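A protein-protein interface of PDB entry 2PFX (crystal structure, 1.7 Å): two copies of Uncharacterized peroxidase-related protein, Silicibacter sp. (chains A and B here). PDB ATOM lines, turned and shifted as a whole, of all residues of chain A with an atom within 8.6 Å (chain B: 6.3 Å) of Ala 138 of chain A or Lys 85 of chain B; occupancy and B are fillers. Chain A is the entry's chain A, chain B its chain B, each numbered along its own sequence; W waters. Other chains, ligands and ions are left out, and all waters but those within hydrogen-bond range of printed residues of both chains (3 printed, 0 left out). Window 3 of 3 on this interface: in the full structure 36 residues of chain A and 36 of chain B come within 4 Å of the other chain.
The backbone carbonyl oxygen (O) of Lys 132 of chain A is in hydrogen-bond range of the backbone NH (N) of Ser 137 of chain A. The side-chain amide oxygen (OD1) of Asn 172 of chain B is in hydrogen-bond range of the side-chain amide nitrogen (ND2) of Asn 84 of chain B, at 2.9 Å. O of Asn 172 of chain B lies close to OG of Ser 176 of chain B (3.3 Å).
Among the printed residues, merely in contact across the chains: Ser 137 of chain A with Ser 176 of chain B, Ala 138 of chain A with Asn 84 of chain B, Ala 138 of chain A with Lys 85 of chain B, Met 133 of chain A with Ala 177 of chain B and Ile 140 of chain A with Ala 177 of chain B.
Ala 138 of chain A touches two residues of chain B. Of chain A, only Ala 138 comes within 4 Å of Lys 85 of chain B. Printed residues of chain A within 4 Å of Ala 177 of chain B: Met 133 (3.7 Å) and Ile 140 (3.7 Å). Printed residues of chain B within 4 Å of Ser 137 of chain A: Ser 176 (3.5 Å). Of the printed residues of chain B, Ile 140 of chain A touches Ala 177. Printed residues of chain B within 4 Å of Met 133 of chain A: Ala 177. The nearest residue of chain B that does not touch Ala 138 of chain A is Ser 176 of chain B (4.3 Å). The nearest residue of chain A that does not touch Lys 85 of chain B is Ser 137 of chain A (6.3 Å).
Printed residues of chain B that touch a printed residue of chain A: Asn 84, Lys 85, Ser 176 and Ala 177. Hydrophobic or aromatic side chains of chain B that line the printed part of chain A: Ala 177. Printed residues of chain A that touch a printed residue of chain B: Met 133, Ser 137, Ala 138 and Ile 140. Among the printed residues, 5 pairs touch across the chains. Among the printed residues, no Asp or Glu carboxylate lies within 4 Å of a Lys or Arg side-chain nitrogen of the other chain.
No position is printed for both chains.
Water W1 lies within hydrogen-bond range of the side-chain hydroxyl of Ser 137 of chain A (2.7 Å), the side-chain hydroxyl of Ser 176 of chain B (2.7 Å), the backbone carbonyl oxygen of Asn 84 of chain B (2.8 Å) and the backbone carbonyl oxygen of Asn 172 of chain B (3.5 Å). Water W2 lies within hydrogen-bond range of O of Asn 84 of chain B (2.8 Å), N of Ala 138 of chain A (3.0 Å) and N of Ser 137 of chain A (3.4 Å). Water W3 lies within hydrogen-bond range of the backbone carbonyl oxygen (O) of Ile 140 of chain A (2.8 Å) and the backbone carbonyl oxygen (O) of Ser 176 of chain B (3.3 Å).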
ATOM      1  N   LYS A 132       9.370 -30.699   9.624  1.00  0.00           N
ATOM      2  CA  LYS A 132       9.024 -29.593   8.749  1.00  0.00           C
ATOM      3  C   LYS A 132       9.121 -28.239   9.442  1.00  0.00           C
ATOM      4  O   LYS A 132       9.495 -27.201   8.863  1.00  0.00           O
ATOM      5  CB  LYS A 132       7.621 -29.815   8.181  1.00  0.00           C
ATOM      6  CG  LYS A 132       7.275 -28.704   7.173  1.00  0.00           C
ATOM      7  CD  LYS A 132       5.918 -28.933   6.522  1.00  0.00           C
ATOM      8  CE  LYS A 132       5.699 -27.874   5.443  1.00  0.00           C
ATOM      9  NZ  LYS A 132       4.656 -28.351   4.500  1.00  0.00           N
ATOM     10  N   MET A 133       8.766 -28.169  10.714  1.00  0.00           N
ATOM     11  CA  MET A 133       8.950 -26.969  11.504  1.00  0.00           C
ATOM     12  C   MET A 133      10.429 -26.617  11.638  1.00  0.00           C
ATOM     13  O   MET A 133      10.833 -25.465  11.648  1.00  0.00           O
ATOM     14  CB  MET A 133       8.414 -27.191  12.912  1.00  0.00           C
ATOM     15  CG  MET A 133       6.917 -27.020  13.078  1.00  0.00           C
ATOM     16  SD  MET A 133       6.325 -27.238  14.857  1.00  0.00           S
ATOM     17  CE  MET A 133       7.225 -25.719  15.580  1.00  0.00           C
ATOM     18  N   THR A 134      11.233 -27.669  11.731  1.00  0.00           N
ATOM     19  CA  THR A 134      12.662 -27.475  11.953  1.00  0.00           C
ATOM     20  C   THR A 134      13.323 -26.962  10.689  1.00  0.00           C
ATOM     21  O   THR A 134      14.130 -26.016  10.718  1.00  0.00           O
ATOM     22  CB  THR A 134      13.282 -28.774  12.484  1.00  0.00           C
ATOM     23  OG1 THR A 134      12.723 -29.041  13.783  1.00  0.00           O
ATOM     24  CG2 THR A 134      14.791 -28.622  12.681  1.00  0.00           C
ATOM     25  N   ARG A 135      12.953 -27.532   9.542  1.00  0.00           N
ATOM     26  CA  ARG A 135      13.519 -27.078   8.269  1.00  0.00           C
ATOM     27  C   ARG A 135      12.840 -25.890   7.617  1.00  0.00           C
ATOM     28  O   ARG A 135      13.472 -25.098   6.888  1.00  0.00           O
ATOM     29  CB  ARG A 135      13.468 -28.269   7.299  1.00  0.00           C
ATOM     30  CG  ARG A 135      14.552 -29.283   7.590  1.00  0.00           C
ATOM     31  CD  ARG A 135      14.036 -30.698   7.690  1.00  0.00           C
ATOM     32  NE  ARG A 135      14.215 -31.433   6.450  1.00  0.00           N
ATOM     33  CZ  ARG A 135      13.930 -32.710   6.260  1.00  0.00           C
ATOM     34  NH1 ARG A 135      13.434 -33.479   7.230  1.00  0.00           N
ATOM     35  NH2 ARG A 135      14.174 -33.190   5.039  1.00  0.00           N
ATOM     36  N   ALA A 136      11.539 -25.720   7.808  1.00  0.00           N
ATOM     37  CA  ALA A 136      10.804 -24.753   6.991  1.00  0.00           C
ATOM     38  C   ALA A 136       9.487 -24.381   7.630  1.00  0.00           C
ATOM     39  O   ALA A 136       8.431 -24.588   7.034  1.00  0.00           O
ATOM     40  CB  ALA A 136      10.553 -25.345   5.615  1.00  0.00           C
ATOM     41  N   SER A 137       9.598 -23.823   8.834  1.00  0.00           N
ATOM     42  CA  SER A 137       8.369 -23.477   9.537  1.00  0.00           C
ATOM     43  C   SER A 137       7.469 -22.527   8.764  1.00  0.00           C
ATOM     44  O   SER A 137       6.244 -22.575   8.911  1.00  0.00           O
ATOM     45  CB  SER A 137       8.714 -22.905  10.923  1.00  0.00           C
ATOM     46  OG  SER A 137       9.515 -21.746  10.873  1.00  0.00           O
ATOM     47  N   ALA A 138       8.047 -21.669   7.919  1.00  0.00           N
ATOM     48  CA  ALA A 138       7.249 -20.690   7.187  1.00  0.00           C
ATOM     49  C   ALA A 138       6.304 -21.353   6.192  1.00  0.00           C
ATOM     50  O   ALA A 138       5.321 -20.756   5.760  1.00  0.00           O
ATOM     51  CB  ALA A 138       8.138 -19.697   6.448  1.00  0.00           C
ATOM     52  N   GLU A 139       6.597 -22.600   5.857  1.00  0.00           N
ATOM     53  CA  GLU A 139       5.801 -23.326   4.882  1.00  0.00           C
ATOM     54  C   GLU A 139       4.745 -24.206   5.528  1.00  0.00           C
ATOM     55  O   GLU A 139       4.004 -24.927   4.874  1.00  0.00           O
ATOM     56  CB  GLU A 139       6.761 -24.168   4.040  1.00  0.00           C
ATOM     57  CG  GLU A 139       7.802 -23.308   3.331  1.00  0.00           C
ATOM     58  CD  GLU A 139       8.676 -24.061   2.361  1.00  0.00           C
ATOM     59  OE1 GLU A 139       8.553 -25.299   2.243  1.00  0.00           O
ATOM     60  OE2 GLU A 139       9.499 -23.380   1.710  1.00  0.00           O
ATOM     61  N   ILE A 140       4.610 -24.188   6.835  1.00  0.00           N
ATOM     62  CA  ILE A 140       3.550 -24.989   7.454  1.00  0.00           C
ATOM     63  C   ILE A 140       2.209 -24.332   7.160  1.00  0.00           C
ATOM     64  O   ILE A 140       2.081 -23.110   7.271  1.00  0.00           O
ATOM     65  CB  ILE A 140       3.746 -25.186   8.947  1.00  0.00           C
ATOM     66  CG1 ILE A 140       4.949 -26.136   9.185  1.00  0.00           C
ATOM     67  CG2 ILE A 140       2.535 -25.707   9.684  1.00  0.00           C
ATOM     68  CD1 ILE A 140       5.617 -25.590  10.418  1.00  0.00           C
ATOM     69  N   GLU A 141       1.255 -25.170   6.759  1.00  0.00           N
ATOM     70  CA  GLU A 141      -0.083 -24.743   6.364  1.00  0.00           C
ATOM     71  C   GLU A 141      -1.184 -25.461   7.158  1.00  0.00           C
ATOM     72  O   GLU A 141      -0.943 -26.441   7.855  1.00  0.00           O
ATOM     73  CB  GLU A 141      -0.418 -25.056   4.906  1.00  0.00           C
ATOM     74  CG  GLU A 141       0.382 -24.432   3.810  1.00  0.00           C
ATOM     75  CD  GLU A 141      -0.151 -23.113   3.295  1.00  0.00           C
ATOM     76  OE1 GLU A 141      -1.370 -22.860   3.305  1.00  0.00           O
ATOM     77  OE2 GLU A 141       0.746 -22.351   2.885  1.00  0.00           O
ATOM     78  N   ASP A 144      -1.215 -29.145   6.935  1.00  0.00           N
ATOM     79  CA  ASP A 144      -0.269 -29.841   7.799  1.00  0.00           C
ATOM     80  C   ASP A 144      -0.825 -30.064   9.196  1.00  0.00           C
ATOM     81  O   ASP A 144      -0.668 -31.094   9.843  1.00  0.00           O
ATOM     82  CB  ASP A 144       1.028 -29.042   7.903  1.00  0.00           C
ATOM     83  CG  ASP A 144       1.742 -28.932   6.570  1.00  0.00           C
ATOM     84  OD1 ASP A 144       1.924 -29.973   5.917  1.00  0.00           O
ATOM     85  OD2 ASP A 144       2.118 -27.841   6.126  1.00  0.00           O
ATOM     86  N   VAL B  80      16.915 -12.958  12.862  1.00  0.00           N
ATOM     87  CA  VAL B  80      16.505 -14.367  12.945  1.00  0.00           C
ATOM     88  C   VAL B  80      15.163 -14.555  12.230  1.00  0.00           C
ATOM     89  O   VAL B  80      15.041 -15.436  11.380  1.00  0.00           O
ATOM     90  CB  VAL B  80      16.438 -14.849  14.391  1.00  0.00           C
ATOM     91  CG1 VAL B  80      15.848 -16.247  14.487  1.00  0.00           C
ATOM     92  CG2 VAL B  80      17.818 -14.814  15.051  1.00  0.00           C
ATOM     93  N   SER B  81      14.167 -13.729  12.531  1.00  0.00           N
ATOM     94  CA  SER B  81      12.836 -13.817  11.946  1.00  0.00           C
ATOM     95  C   SER B  81      12.786 -13.634  10.442  1.00  0.00           C
ATOM     96  O   SER B  81      11.967 -14.195   9.728  1.00  0.00           O
ATOM     97  CB  SER B  81      11.928 -12.730  12.502  1.00  0.00           C
ATOM     98  OG  SER B  81      11.968 -12.596  13.890  1.00  0.00           O
ATOM     99  N   SER B  82      13.675 -12.774   9.945  1.00  0.00           N
ATOM    100  CA  SER B  82      13.757 -12.585   8.504  1.00  0.00           C
ATOM    101  C   SER B  82      14.196 -13.869   7.829  1.00  0.00           C
ATOM    102  O   SER B  82      13.701 -14.299   6.796  1.00  0.00           O
ATOM    103  CB  SER B  82      14.741 -11.442   8.200  1.00  0.00           C
ATOM    104  OG  SER B  82      14.943 -11.279   6.822  1.00  0.00           O
ATOM    105  N   ILE B  83      15.207 -14.511   8.426  1.00  0.00           N
ATOM    106  CA  ILE B  83      15.728 -15.729   7.813  1.00  0.00           C
ATOM    107  C   ILE B  83      14.692 -16.831   7.865  1.00  0.00           C
ATOM    108  O   ILE B  83      14.546 -17.626   6.930  1.00  0.00           O
ATOM    109  CB  ILE B  83      17.027 -16.202   8.509  1.00  0.00           C
ATOM    110  CG1 ILE B  83      18.184 -15.228   8.350  1.00  0.00           C
ATOM    111  CG2 ILE B  83      17.355 -17.619   8.025  1.00  0.00           C
ATOM    112  CD1 ILE B  83      19.387 -15.455   9.251  1.00  0.00           C
ATOM    113  N   ASN B  84      13.958 -16.864   8.974  1.00  0.00           N
ATOM    114  CA  ASN B  84      12.914 -17.876   9.079  1.00  0.00           C
ATOM    115  C   ASN B  84      11.581 -17.448   8.462  1.00  0.00           C
ATOM    116  O   ASN B  84      10.647 -18.272   8.457  1.00  0.00           O
ATOM    117  CB  ASN B  84      12.652 -18.251  10.538  1.00  0.00           C
ATOM    118  CG  ASN B  84      13.852 -18.984  11.119  1.00  0.00           C
ATOM    119  OD1 ASN B  84      14.516 -19.736  10.413  1.00  0.00           O
ATOM    120  ND2 ASN B  84      14.102 -18.740  12.393  1.00  0.00           N
ATOM    121  N   LYS B  85      11.496 -16.228   7.979  1.00  0.00           N
ATOM    122  CA  LYS B  85      10.293 -15.728   7.315  1.00  0.00           C
ATOM    123  C   LYS B  85       9.064 -15.833   8.214  1.00  0.00           C
ATOM    124  O   LYS B  85       7.984 -16.285   7.822  1.00  0.00           O
ATOM    125  CB  LYS B  85      10.054 -16.469   5.996  1.00  0.00           C
ATOM    126  CG  LYS B  85      11.271 -16.460   5.066  1.00  0.00           C
ATOM    127  CD  LYS B  85      10.910 -16.601   3.601  1.00  0.00           C
ATOM    128  CE  LYS B  85      10.918 -15.295   2.818  1.00  0.00           C
ATOM    129  NZ  LYS B  85       9.529 -14.879   2.458  1.00  0.00           N
ATOM    130  N   CYS B  86       9.261 -15.396   9.456  1.00  0.00           N
ATOM    131  CA  CYS B  86       8.219 -15.400  10.461  1.00  0.00           C
ATOM    132  C   CYS B  86       7.419 -14.108  10.474  1.00  0.00           C
ATOM    133  O   CYS B  86       7.907 -13.072  10.929  1.00  0.00           O
ATOM    134  CB  CYS B  86       8.809 -15.607  11.868  1.00  0.00           C
ATOM    135  SG  CYS B  86       7.438 -15.770  13.034  1.00  0.00           S
ATOM    136  N   PHE B  87       6.190 -14.120   9.952  1.00  0.00           N
ATOM    137  CA  PHE B  87       5.385 -12.907   9.860  1.00  0.00           C
ATOM    138  C   PHE B  87       5.114 -12.245  11.218  1.00  0.00           C
ATOM    139  O   PHE B  87       5.302 -11.024  11.344  1.00  0.00           O
ATOM    140  CB  PHE B  87       4.066 -13.220   9.166  1.00  0.00           C
ATOM    141  CG  PHE B  87       3.063 -12.092   9.071  1.00  0.00           C
ATOM    142  CD1 PHE B  87       3.359 -10.920   8.388  1.00  0.00           C
ATOM    143  CD2 PHE B  87       1.815 -12.208   9.673  1.00  0.00           C
ATOM    144  CE1 PHE B  87       2.442  -9.894   8.300  1.00  0.00           C
ATOM    145  CE2 PHE B  87       0.899 -11.177   9.575  1.00  0.00           C
ATOM    146  CZ  PHE B  87       1.197 -10.012   8.890  1.00  0.00           C
ATOM    147  N   LEU B  90       8.396 -10.732  12.554  1.00  0.00           N
ATOM    148  CA  LEU B  90       8.885  -9.625  11.724  1.00  0.00           C
ATOM    149  C   LEU B  90       8.068  -8.374  11.943  1.00  0.00           C
ATOM    150  O   LEU B  90       8.574  -7.259  11.871  1.00  0.00           O
ATOM    151  CB  LEU B  90       8.871  -9.991  10.229  1.00  0.00           C
ATOM    152  CG  LEU B  90       9.981 -10.944   9.762  1.00  0.00           C
ATOM    153  CD1 LEU B  90       9.680 -11.493   8.383  1.00  0.00           C
ATOM    154  CD2 LEU B  90      11.335 -10.254   9.776  1.00  0.00           C
ATOM    155  N   ASN B 172       9.814 -18.133  16.417  1.00  0.00           N
ATOM    156  CA  ASN B 172       9.418 -18.114  15.014  1.00  0.00           C
ATOM    157  C   ASN B 172       8.688 -19.380  14.604  1.00  0.00           C
ATOM    158  O   ASN B 172       7.758 -19.298  13.833  1.00  0.00           O
ATOM    159  CB  ASN B 172      10.655 -18.003  14.117  1.00  0.00           C
ATOM    160  CG  ASN B 172      11.448 -16.727  14.179  1.00  0.00           C
ATOM    161  OD1 ASN B 172      12.477 -16.556  13.505  1.00  0.00           O
ATOM    162  ND2 ASN B 172      10.988 -15.840  15.030  1.00  0.00           N
ATOM    163  N   SER B 176       4.898 -19.520  13.390  1.00  0.00           N
ATOM    164  CA  SER B 176       4.628 -19.909  12.020  1.00  0.00           C
ATOM    165  C   SER B 176       3.839 -21.204  12.007  1.00  0.00           C
ATOM    166  O   SER B 176       2.892 -21.312  11.225  1.00  0.00           O
ATOM    167  CB  SER B 176       5.930 -20.029  11.231  1.00  0.00           C
ATOM    168  OG  SER B 176       6.378 -18.724  10.858  1.00  0.00           O
ATOM    169  N   ALA B 177       4.200 -22.157  12.846  1.00  0.00           N
ATOM    170  CA  ALA B 177       3.479 -23.427  12.783  1.00  0.00           C
ATOM    171  C   ALA B 177       2.033 -23.308  13.209  1.00  0.00           C
ATOM    172  O   ALA B 177       1.219 -24.156  12.814  1.00  0.00           O
ATOM    173  CB  ALA B 177       4.164 -24.459  13.664  1.00  0.00           C
HETATM  174  O   HOH W   1       9.086 -19.059  10.625  1.00  0.00           O
HETATM  175  O   HOH W   2      10.989 -20.957   7.665  1.00  0.00           O
HETATM  176  O   HOH W   3       0.361 -21.896   9.180  1.00  0.00           O
